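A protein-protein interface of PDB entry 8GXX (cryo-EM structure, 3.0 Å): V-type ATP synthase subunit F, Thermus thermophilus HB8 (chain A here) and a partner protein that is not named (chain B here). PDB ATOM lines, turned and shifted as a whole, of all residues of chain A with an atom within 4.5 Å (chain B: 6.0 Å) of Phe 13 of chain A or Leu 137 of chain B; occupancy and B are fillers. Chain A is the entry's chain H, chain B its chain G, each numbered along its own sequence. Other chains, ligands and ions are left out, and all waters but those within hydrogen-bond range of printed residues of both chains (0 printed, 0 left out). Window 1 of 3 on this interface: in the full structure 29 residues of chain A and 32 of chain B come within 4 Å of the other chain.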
ATOM      1  N   VAL A   3     -16.500 -17.983   4.477  1.00  0.00           N
ATOM      2  CA  VAL A   3     -16.895 -16.704   5.053  1.00  0.00           C
ATOM      3  C   VAL A   3     -17.366 -15.800   3.928  1.00  0.00           C
ATOM      4  O   VAL A   3     -16.706 -15.700   2.889  1.00  0.00           O
ATOM      5  CB  VAL A   3     -15.740 -16.043   5.823  1.00  0.00           C
ATOM      6  CG1 VAL A   3     -16.161 -14.671   6.328  1.00  0.00           C
ATOM      7  CG2 VAL A   3     -15.294 -16.938   6.968  1.00  0.00           C
ATOM      8  N   THR A   9     -11.539  -9.644   1.481  1.00  0.00           N
ATOM      9  CA  THR A   9     -11.321 -10.823   2.307  1.00  0.00           C
ATOM     10  C   THR A   9     -11.923 -12.079   1.699  1.00  0.00           C
ATOM     11  O   THR A   9     -11.534 -13.185   2.088  1.00  0.00           O
ATOM     12  CB  THR A   9     -11.904 -10.619   3.708  1.00  0.00           C
ATOM     13  OG1 THR A   9     -11.655 -11.784   4.503  1.00  0.00           O
ATOM     14  CG2 THR A   9     -13.406 -10.370   3.642  1.00  0.00           C
ATOM     15  N   ALA A  10     -12.861 -11.940   0.760  1.00  0.00           N
ATOM     16  CA  ALA A  10     -13.449 -13.120   0.138  1.00  0.00           C
ATOM     17  C   ALA A  10     -12.368 -13.991  -0.484  1.00  0.00           C
ATOM     18  O   ALA A  10     -12.325 -15.204  -0.260  1.00  0.00           O
ATOM     19  CB  ALA A  10     -14.480 -12.698  -0.909  1.00  0.00           C
ATOM     20  N   GLN A  11     -11.477 -13.382  -1.266  1.00  0.00           N
ATOM     21  CA  GLN A  11     -10.315 -14.103  -1.769  1.00  0.00           C
ATOM     22  C   GLN A  11      -9.253 -14.284  -0.693  1.00  0.00           C
ATOM     23  O   GLN A  11      -8.456 -15.224  -0.769  1.00  0.00           O
ATOM     24  CB  GLN A  11      -9.719 -13.365  -2.968  1.00  0.00           C
ATOM     25  CG  GLN A  11      -9.213 -11.966  -2.650  1.00  0.00           C
ATOM     26  CD  GLN A  11      -8.675 -11.248  -3.872  1.00  0.00           C
ATOM     27  OE1 GLN A  11      -8.884 -11.682  -5.004  1.00  0.00           O
ATOM     28  NE2 GLN A  11      -7.975 -10.142  -3.647  1.00  0.00           N
ATOM     29  N   GLY A  12      -9.224 -13.402   0.307  1.00  0.00           N
ATOM     30  CA  GLY A  12      -8.226 -13.527   1.356  1.00  0.00           C
ATOM     31  C   GLY A  12      -8.342 -14.836   2.112  1.00  0.00           C
ATOM     32  O   GLY A  12      -7.338 -15.430   2.506  1.00  0.00           O
ATOM     33  N   PHE A  13      -9.570 -15.296   2.339  1.00  0.00           N
ATOM     34  CA  PHE A  13      -9.744 -16.576   3.012  1.00  0.00           C
ATOM     35  C   PHE A  13      -9.189 -17.715   2.167  1.00  0.00           C
ATOM     36  O   PHE A  13      -8.584 -18.653   2.699  1.00  0.00           O
ATOM     37  CB  PHE A  13     -11.216 -16.806   3.344  1.00  0.00           C
ATOM     38  CG  PHE A  13     -11.611 -16.285   4.693  1.00  0.00           C
ATOM     39  CD1 PHE A  13     -11.531 -17.096   5.811  1.00  0.00           C
ATOM     40  CD2 PHE A  13     -12.045 -14.980   4.848  1.00  0.00           C
ATOM     41  CE1 PHE A  13     -11.885 -16.620   7.056  1.00  0.00           C
ATOM     42  CE2 PHE A  13     -12.400 -14.497   6.089  1.00  0.00           C
ATOM     43  CZ  PHE A  13     -12.320 -15.318   7.195  1.00  0.00           C
ATOM     44  N   ARG A  14      -9.370 -17.645   0.848  1.00  0.00           N
ATOM     45  CA  ARG A  14      -8.704 -18.603  -0.024  1.00  0.00           C
ATOM     46  C   ARG A  14      -7.196 -18.490   0.126  1.00  0.00           C
ATOM     47  O   ARG A  14      -6.485 -19.501   0.146  1.00  0.00           O
ATOM     48  CB  ARG A  14      -9.122 -18.375  -1.477  1.00  0.00           C
ATOM     49  CG  ARG A  14      -8.633 -19.447  -2.443  1.00  0.00           C
ATOM     50  CD  ARG A  14      -9.400 -20.750  -2.278  1.00  0.00           C
ATOM     51  NE  ARG A  14     -10.765 -20.651  -2.781  1.00  0.00           N
ATOM     52  CZ  ARG A  14     -11.124 -20.892  -4.036  1.00  0.00           C
ATOM     53  NH1 ARG A  14     -10.240 -21.245  -4.955  1.00  0.00           N
ATOM     54  NH2 ARG A  14     -12.405 -20.775  -4.377  1.00  0.00           N
ATOM     55  N   LEU A  15      -6.694 -17.260   0.237  1.00  0.00           N
ATOM     56  CA  LEU A  15      -5.283 -17.054   0.527  1.00  0.00           C
ATOM     57  C   LEU A  15      -4.892 -17.693   1.849  1.00  0.00           C
ATOM     58  O   LEU A  15      -3.710 -17.983   2.063  1.00  0.00           O
ATOM     59  CB  LEU A  15      -4.956 -15.559   0.553  1.00  0.00           C
ATOM     60  CG  LEU A  15      -3.493 -15.185   0.799  1.00  0.00           C
ATOM     61  CD1 LEU A  15      -2.617 -15.645  -0.357  1.00  0.00           C
ATOM     62  CD2 LEU A  15      -3.352 -13.686   1.021  1.00  0.00           C
ATOM     63  N   ALA A  16      -5.856 -17.916   2.734  1.00  0.00           N
ATOM     64  CA  ALA A  16      -5.616 -18.594   4.000  1.00  0.00           C
ATOM     65  C   ALA A  16      -5.798 -20.102   3.908  1.00  0.00           C
ATOM     66  O   ALA A  16      -5.658 -20.790   4.924  1.00  0.00           O
ATOM     67  CB  ALA A  16      -6.551 -18.039   5.076  1.00  0.00           C
ATOM     68  N   GLY A  17      -6.107 -20.632   2.726  1.00  0.00           N
ATOM     69  CA  GLY A  17      -6.427 -22.035   2.578  1.00  0.00           C
ATOM     70  C   GLY A  17      -7.873 -22.378   2.851  1.00  0.00           C
ATOM     71  O   GLY A  17      -8.265 -23.536   2.663  1.00  0.00           O
ATOM     72  N   LEU A  18      -8.671 -21.413   3.291  1.00  0.00           N
ATOM     73  CA  LEU A  18     -10.091 -21.586   3.529  1.00  0.00           C
ATOM     74  C   LEU A  18     -10.860 -21.190   2.272  1.00  0.00           C
ATOM     75  O   LEU A  18     -10.297 -21.086   1.179  1.00  0.00           O
ATOM     76  CB  LEU A  18     -10.516 -20.768   4.749  1.00  0.00           C
ATOM     77  CG  LEU A  18      -9.714 -21.037   6.026  1.00  0.00           C
ATOM     78  CD1 LEU A  18     -10.227 -20.181   7.172  1.00  0.00           C
ATOM     79  CD2 LEU A  18      -9.759 -22.513   6.393  1.00  0.00           C
ATOM     80  N   GLU A  19     -12.166 -20.990   2.416  1.00  0.00           N
ATOM     81  CA  GLU A  19     -13.020 -20.556   1.324  1.00  0.00           C
ATOM     82  C   GLU A  19     -13.666 -19.225   1.675  1.00  0.00           C
ATOM     83  O   GLU A  19     -13.885 -18.913   2.849  1.00  0.00           O
ATOM     84  CB  GLU A  19     -14.098 -21.598   1.016  1.00  0.00           C
ATOM     85  CG  GLU A  19     -13.534 -22.901   0.473  1.00  0.00           C
ATOM     86  CD  GLU A  19     -14.595 -23.962   0.278  1.00  0.00           C
ATOM     87  OE1 GLU A  19     -15.741 -23.741   0.718  1.00  0.00           O
ATOM     88  OE2 GLU A  19     -14.283 -25.015  -0.316  1.00  0.00           O
ATOM     89  N   GLY A  20     -13.961 -18.439   0.645  1.00  0.00           N
ATOM     90  CA  GLY A  20     -14.594 -17.151   0.844  1.00  0.00           C
ATOM     91  C   GLY A  20     -15.473 -16.797  -0.333  1.00  0.00           C
ATOM     92  O   GLY A  20     -15.293 -17.299  -1.447  1.00  0.00           O
ATOM     93  N   ILE A  74     -19.554 -11.399  12.067  1.00  0.00           N
ATOM     94  CA  ILE A  74     -18.234 -10.806  12.227  1.00  0.00           C
ATOM     95  C   ILE A  74     -18.255  -9.393  11.662  1.00  0.00           C
ATOM     96  O   ILE A  74     -19.224  -8.958  11.038  1.00  0.00           O
ATOM     97  CB  ILE A  74     -17.129 -11.640  11.552  1.00  0.00           C
ATOM     98  CG1 ILE A  74     -17.563 -12.062  10.151  1.00  0.00           C
ATOM     99  CG2 ILE A  74     -16.810 -12.861  12.386  1.00  0.00           C
ATOM    100  CD1 ILE A  74     -16.478 -12.752   9.363  1.00  0.00           C
ATOM    101  N   LEU B  53      -9.747 -11.350  18.681  1.00  0.00           N
ATOM    102  CA  LEU B  53     -10.119 -11.468  17.278  1.00  0.00           C
ATOM    103  C   LEU B  53     -10.126 -10.110  16.599  1.00  0.00           C
ATOM    104  O   LEU B  53      -9.760 -10.002  15.430  1.00  0.00           O
ATOM    105  CB  LEU B  53     -11.489 -12.126  17.148  1.00  0.00           C
ATOM    106  CG  LEU B  53     -11.986 -12.297  15.711  1.00  0.00           C
ATOM    107  CD1 LEU B  53     -11.140 -13.318  14.980  1.00  0.00           C
ATOM    108  CD2 LEU B  53     -13.453 -12.692  15.688  1.00  0.00           C
ATOM    109  N   PHE B 130      -3.965 -14.220   7.886  1.00  0.00           N
ATOM    110  CA  PHE B 130      -5.308 -14.774   7.759  1.00  0.00           C
ATOM    111  C   PHE B 130      -5.420 -16.145   8.409  1.00  0.00           C
ATOM    112  O   PHE B 130      -6.492 -16.504   8.893  1.00  0.00           O
ATOM    113  CB  PHE B 130      -5.722 -14.854   6.295  1.00  0.00           C
ATOM    114  CG  PHE B 130      -6.016 -13.525   5.677  1.00  0.00           C
ATOM    115  CD1 PHE B 130      -7.178 -12.850   5.989  1.00  0.00           C
ATOM    116  CD2 PHE B 130      -5.135 -12.956   4.776  1.00  0.00           C
ATOM    117  CE1 PHE B 130      -7.457 -11.630   5.424  1.00  0.00           C
ATOM    118  CE2 PHE B 130      -5.406 -11.733   4.205  1.00  0.00           C
ATOM    119  CZ  PHE B 130      -6.571 -11.068   4.531  1.00  0.00           C
ATOM    120  N   ARG B 132      -3.774 -17.121  11.223  1.00  0.00           N
ATOM    121  CA  ARG B 132      -3.946 -16.836  12.646  1.00  0.00           C
ATOM    122  C   ARG B 132      -5.319 -16.228  12.917  1.00  0.00           C
ATOM    123  O   ARG B 132      -5.950 -16.516  13.943  1.00  0.00           O
ATOM    124  CB  ARG B 132      -2.830 -15.915  13.132  1.00  0.00           C
ATOM    125  CG  ARG B 132      -1.457 -16.571  13.091  1.00  0.00           C
ATOM    126  CD  ARG B 132      -0.364 -15.663  13.633  1.00  0.00           C
ATOM    127  NE  ARG B 132      -0.004 -14.604  12.696  1.00  0.00           N
ATOM    128  CZ  ARG B 132      -0.531 -13.387  12.690  1.00  0.00           C
ATOM    129  NH1 ARG B 132      -1.467 -13.030  13.555  1.00  0.00           N
ATOM    130  NH2 ARG B 132      -0.107 -12.502  11.791  1.00  0.00           N
ATOM    131  N   TYR B 133      -5.808 -15.402  11.990  1.00  0.00           N
ATOM    132  CA  TYR B 133      -7.165 -14.885  12.091  1.00  0.00           C
ATOM    133  C   TYR B 133      -8.182 -16.018  12.074  1.00  0.00           C
ATOM    134  O   TYR B 133      -9.187 -15.973  12.789  1.00  0.00           O
ATOM    135  CB  TYR B 133      -7.416 -13.912  10.947  1.00  0.00           C
ATOM    136  CG  TYR B 133      -8.838 -13.447  10.816  1.00  0.00           C
ATOM    137  CD1 TYR B 133      -9.446 -12.725  11.826  1.00  0.00           C
ATOM    138  CD2 TYR B 133      -9.563 -13.702   9.664  1.00  0.00           C
ATOM    139  CE1 TYR B 133     -10.747 -12.287  11.701  1.00  0.00           C
ATOM    140  CE2 TYR B 133     -10.859 -13.267   9.528  1.00  0.00           C
ATOM    141  CZ  TYR B 133     -11.449 -12.561  10.550  1.00  0.00           C
ATOM    142  OH  TYR B 133     -12.748 -12.125  10.421  1.00  0.00           O
ATOM    143  N   ALA B 134      -7.938 -17.041  11.258  1.00  0.00           N
ATOM    144  CA  ALA B 134      -8.834 -18.188  11.213  1.00  0.00           C
ATOM    145  C   ALA B 134      -8.828 -18.936  12.535  1.00  0.00           C
ATOM    146  O   ALA B 134      -9.877 -19.397  13.002  1.00  0.00           O
ATOM    147  CB  ALA B 134      -8.431 -19.118  10.072  1.00  0.00           C
ATOM    148  N   GLU B 135      -7.655 -19.085  13.145  1.00  0.00           N
ATOM    149  CA  GLU B 135      -7.601 -19.723  14.457  1.00  0.00           C
ATOM    150  C   GLU B 135      -8.404 -18.922  15.480  1.00  0.00           C
ATOM    151  O   GLU B 135      -9.153 -19.492  16.293  1.00  0.00           O
ATOM    152  CB  GLU B 135      -6.145 -19.874  14.902  1.00  0.00           C
ATOM    153  CG  GLU B 135      -5.946 -20.743  16.137  1.00  0.00           C
ATOM    154  CD  GLU B 135      -6.238 -20.014  17.436  1.00  0.00           C
ATOM    155  OE1 GLU B 135      -6.275 -18.764  17.427  1.00  0.00           O
ATOM    156  OE2 GLU B 135      -6.429 -20.691  18.467  1.00  0.00           O
ATOM    157  N   ALA B 136      -8.263 -17.595  15.447  1.00  0.00           N
ATOM    158  CA  ALA B 136      -9.047 -16.750  16.339  1.00  0.00           C
ATOM    159  C   ALA B 136     -10.537 -16.927  16.084  1.00  0.00           C
ATOM    160  O   ALA B 136     -11.335 -16.992  17.028  1.00  0.00           O
ATOM    161  CB  ALA B 136      -8.643 -15.288  16.163  1.00  0.00           C
ATOM    162  N   LEU B 137     -10.929 -17.013  14.813  1.00  0.00           N
ATOM    163  CA  LEU B 137     -12.326 -17.260  14.469  1.00  0.00           C
ATOM    164  C   LEU B 137     -12.810 -18.572  15.068  1.00  0.00           C
ATOM    165  O   LEU B 137     -13.926 -18.655  15.592  1.00  0.00           O
ATOM    166  CB  LEU B 137     -12.497 -17.295  12.954  1.00  0.00           C
ATOM    167  CG  LEU B 137     -12.330 -16.000  12.165  1.00  0.00           C
ATOM    168  CD1 LEU B 137     -12.415 -16.306  10.677  1.00  0.00           C
ATOM    169  CD2 LEU B 137     -13.380 -14.982  12.565  1.00  0.00           C
ATOM    170  N   ILE B 138     -11.996 -19.618  14.969  1.00  0.00           N
ATOM    171  CA  ILE B 138     -12.398 -20.919  15.499  1.00  0.00           C
ATOM    172  C   ILE B 138     -12.663 -20.816  16.994  1.00  0.00           C
ATOM    173  O   ILE B 138     -13.703 -21.266  17.498  1.00  0.00           O
ATOM    174  CB  ILE B 138     -11.324 -21.976  15.197  1.00  0.00           C
ATOM    175  CG1 ILE B 138     -11.234 -22.230  13.692  1.00  0.00           C
ATOM    176  CG2 ILE B 138     -11.634 -23.265  15.943  1.00  0.00           C
ATOM    177  CD1 ILE B 138      -9.941 -22.902  13.263  1.00  0.00           C
ATOM    178  N   ARG B 139     -11.728 -20.211  17.727  1.00  0.00           N
ATOM    179  CA  ARG B 139     -11.921 -20.099  19.169  1.00  0.00           C
ATOM    180  C   ARG B 139     -13.162 -19.273  19.492  1.00  0.00           C
ATOM    181  O   ARG B 139     -13.929 -19.615  20.407  1.00  0.00           O
ATOM    182  CB  ARG B 139     -10.681 -19.493  19.826  1.00  0.00           C
ATOM    183  CG  ARG B 139     -10.569 -19.826  21.307  1.00  0.00           C
ATOM    184  CD  ARG B 139      -9.292 -19.289  21.940  1.00  0.00           C
ATOM    185  NE  ARG B 139      -9.448 -17.926  22.442  1.00  0.00           N
ATOM    186  CZ  ARG B 139      -8.622 -16.917  22.186  1.00  0.00           C
ATOM    187  NH1 ARG B 139      -7.545 -17.070  21.433  1.00  0.00           N
ATOM    188  NH2 ARG B 139      -8.881 -15.723  22.709  1.00  0.00           N
ATOM    189  N   VAL B 140     -13.375 -18.179  18.759  1.00  0.00           N
ATOM    190  CA  VAL B 140     -14.515 -17.311  19.034  1.00  0.00           C
ATOM    191  C   VAL B 140     -15.820 -18.052  18.789  1.00  0.00           C
ATOM    192  O   VAL B 140     -16.775 -17.936  19.567  1.00  0.00           O
ATOM    193  CB  VAL B 140     -14.424 -16.032  18.186  1.00  0.00           C
ATOM    194  CG1 VAL B 140     -15.727 -15.263  18.250  1.00  0.00           C
ATOM    195  CG2 VAL B 140     -13.271 -15.168  18.669  1.00  0.00           C
ATOM    196  N   ALA B 141     -15.890 -18.810  17.698  1.00  0.00           N
ATOM    197  CA  ALA B 141     -17.090 -19.591  17.428  1.00  0.00           C
ATOM    198  C   ALA B 141     -17.340 -20.587  18.545  1.00  0.00           C
ATOM    199  O   ALA B 141     -18.479 -20.750  19.001  1.00  0.00           O
ATOM    200  CB  ALA B 141     -16.957 -20.310  16.088  1.00  0.00           C
ATOM    201  N   ASN B 142     -16.284 -21.257  19.006  1.00  0.00           N
ATOM    202  CA  ASN B 142     -16.447 -22.215  20.091  1.00  0.00           C
ATOM    203  C   ASN B 142     -17.057 -21.552  21.318  1.00  0.00           C
ATOM    204  O   ASN B 142     -18.066 -22.026  21.862  1.00  0.00           O
ATOM    205  CB  ASN B 142     -15.099 -22.837  20.429  1.00  0.00           C
ATOM    206  CG  ASN B 142     -14.517 -23.606  19.275  1.00  0.00           C
ATOM    207  OD1 ASN B 142     -14.928 -23.432  18.130  1.00  0.00           O
ATOM    208  ND2 ASN B 142     -13.559 -24.475  19.566  1.00  0.00           N
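Among the printed residues, pairs that only touch across the chains: Phe 13 of chain A with Tyr 133 of chain B (3.4 Å), Ala 16 of chain A with Phe 130 of chain B (3.5 Å), Leu 18 of chain A with Ala 134 of chain B (3.6 Å), Phe 13 of chain A with Leu 137 of chain B (3.6 Å), Ile 74 of chain A with Tyr 133 of chain B (3.9 Å) and Gly 12 of chain A with Phe 130 of chain B (3.9 Å).
The backbone carbonyl oxygen (O) of Phe 13 of chain A lies within hydrogen-bond range of the backbone NH (N) of Leu 18 of chain A, at 2.8 Å.
Thr 9 of chain A touches none of the printed residues of chain B.
Of chain B, only Tyr 133 and Leu 137 come within 4 Å of Phe 13 of chain A.
Of the printed residues of chain B, Ala 16 of chain A touches Phe 130 (3.5 Å).
Of the printed residues of chain A, Ala 134 of chain B touches Leu 18 (3.6 Å).
Printed residues of chain A within 4 Å of Leu 137 of chain B: Phe 13 (3.6 Å).
The nearest residue of chain B that does not touch Phe 13 of chain A is Phe 130 of chain B (5.0 Å).
Hydrophobic or aromatic side chains of chain A that line the printed part of chain B: Phe 13, Ala 16, Leu 18 and Ile 74.
Among the printed residues, 6 pairs touch across the chains.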
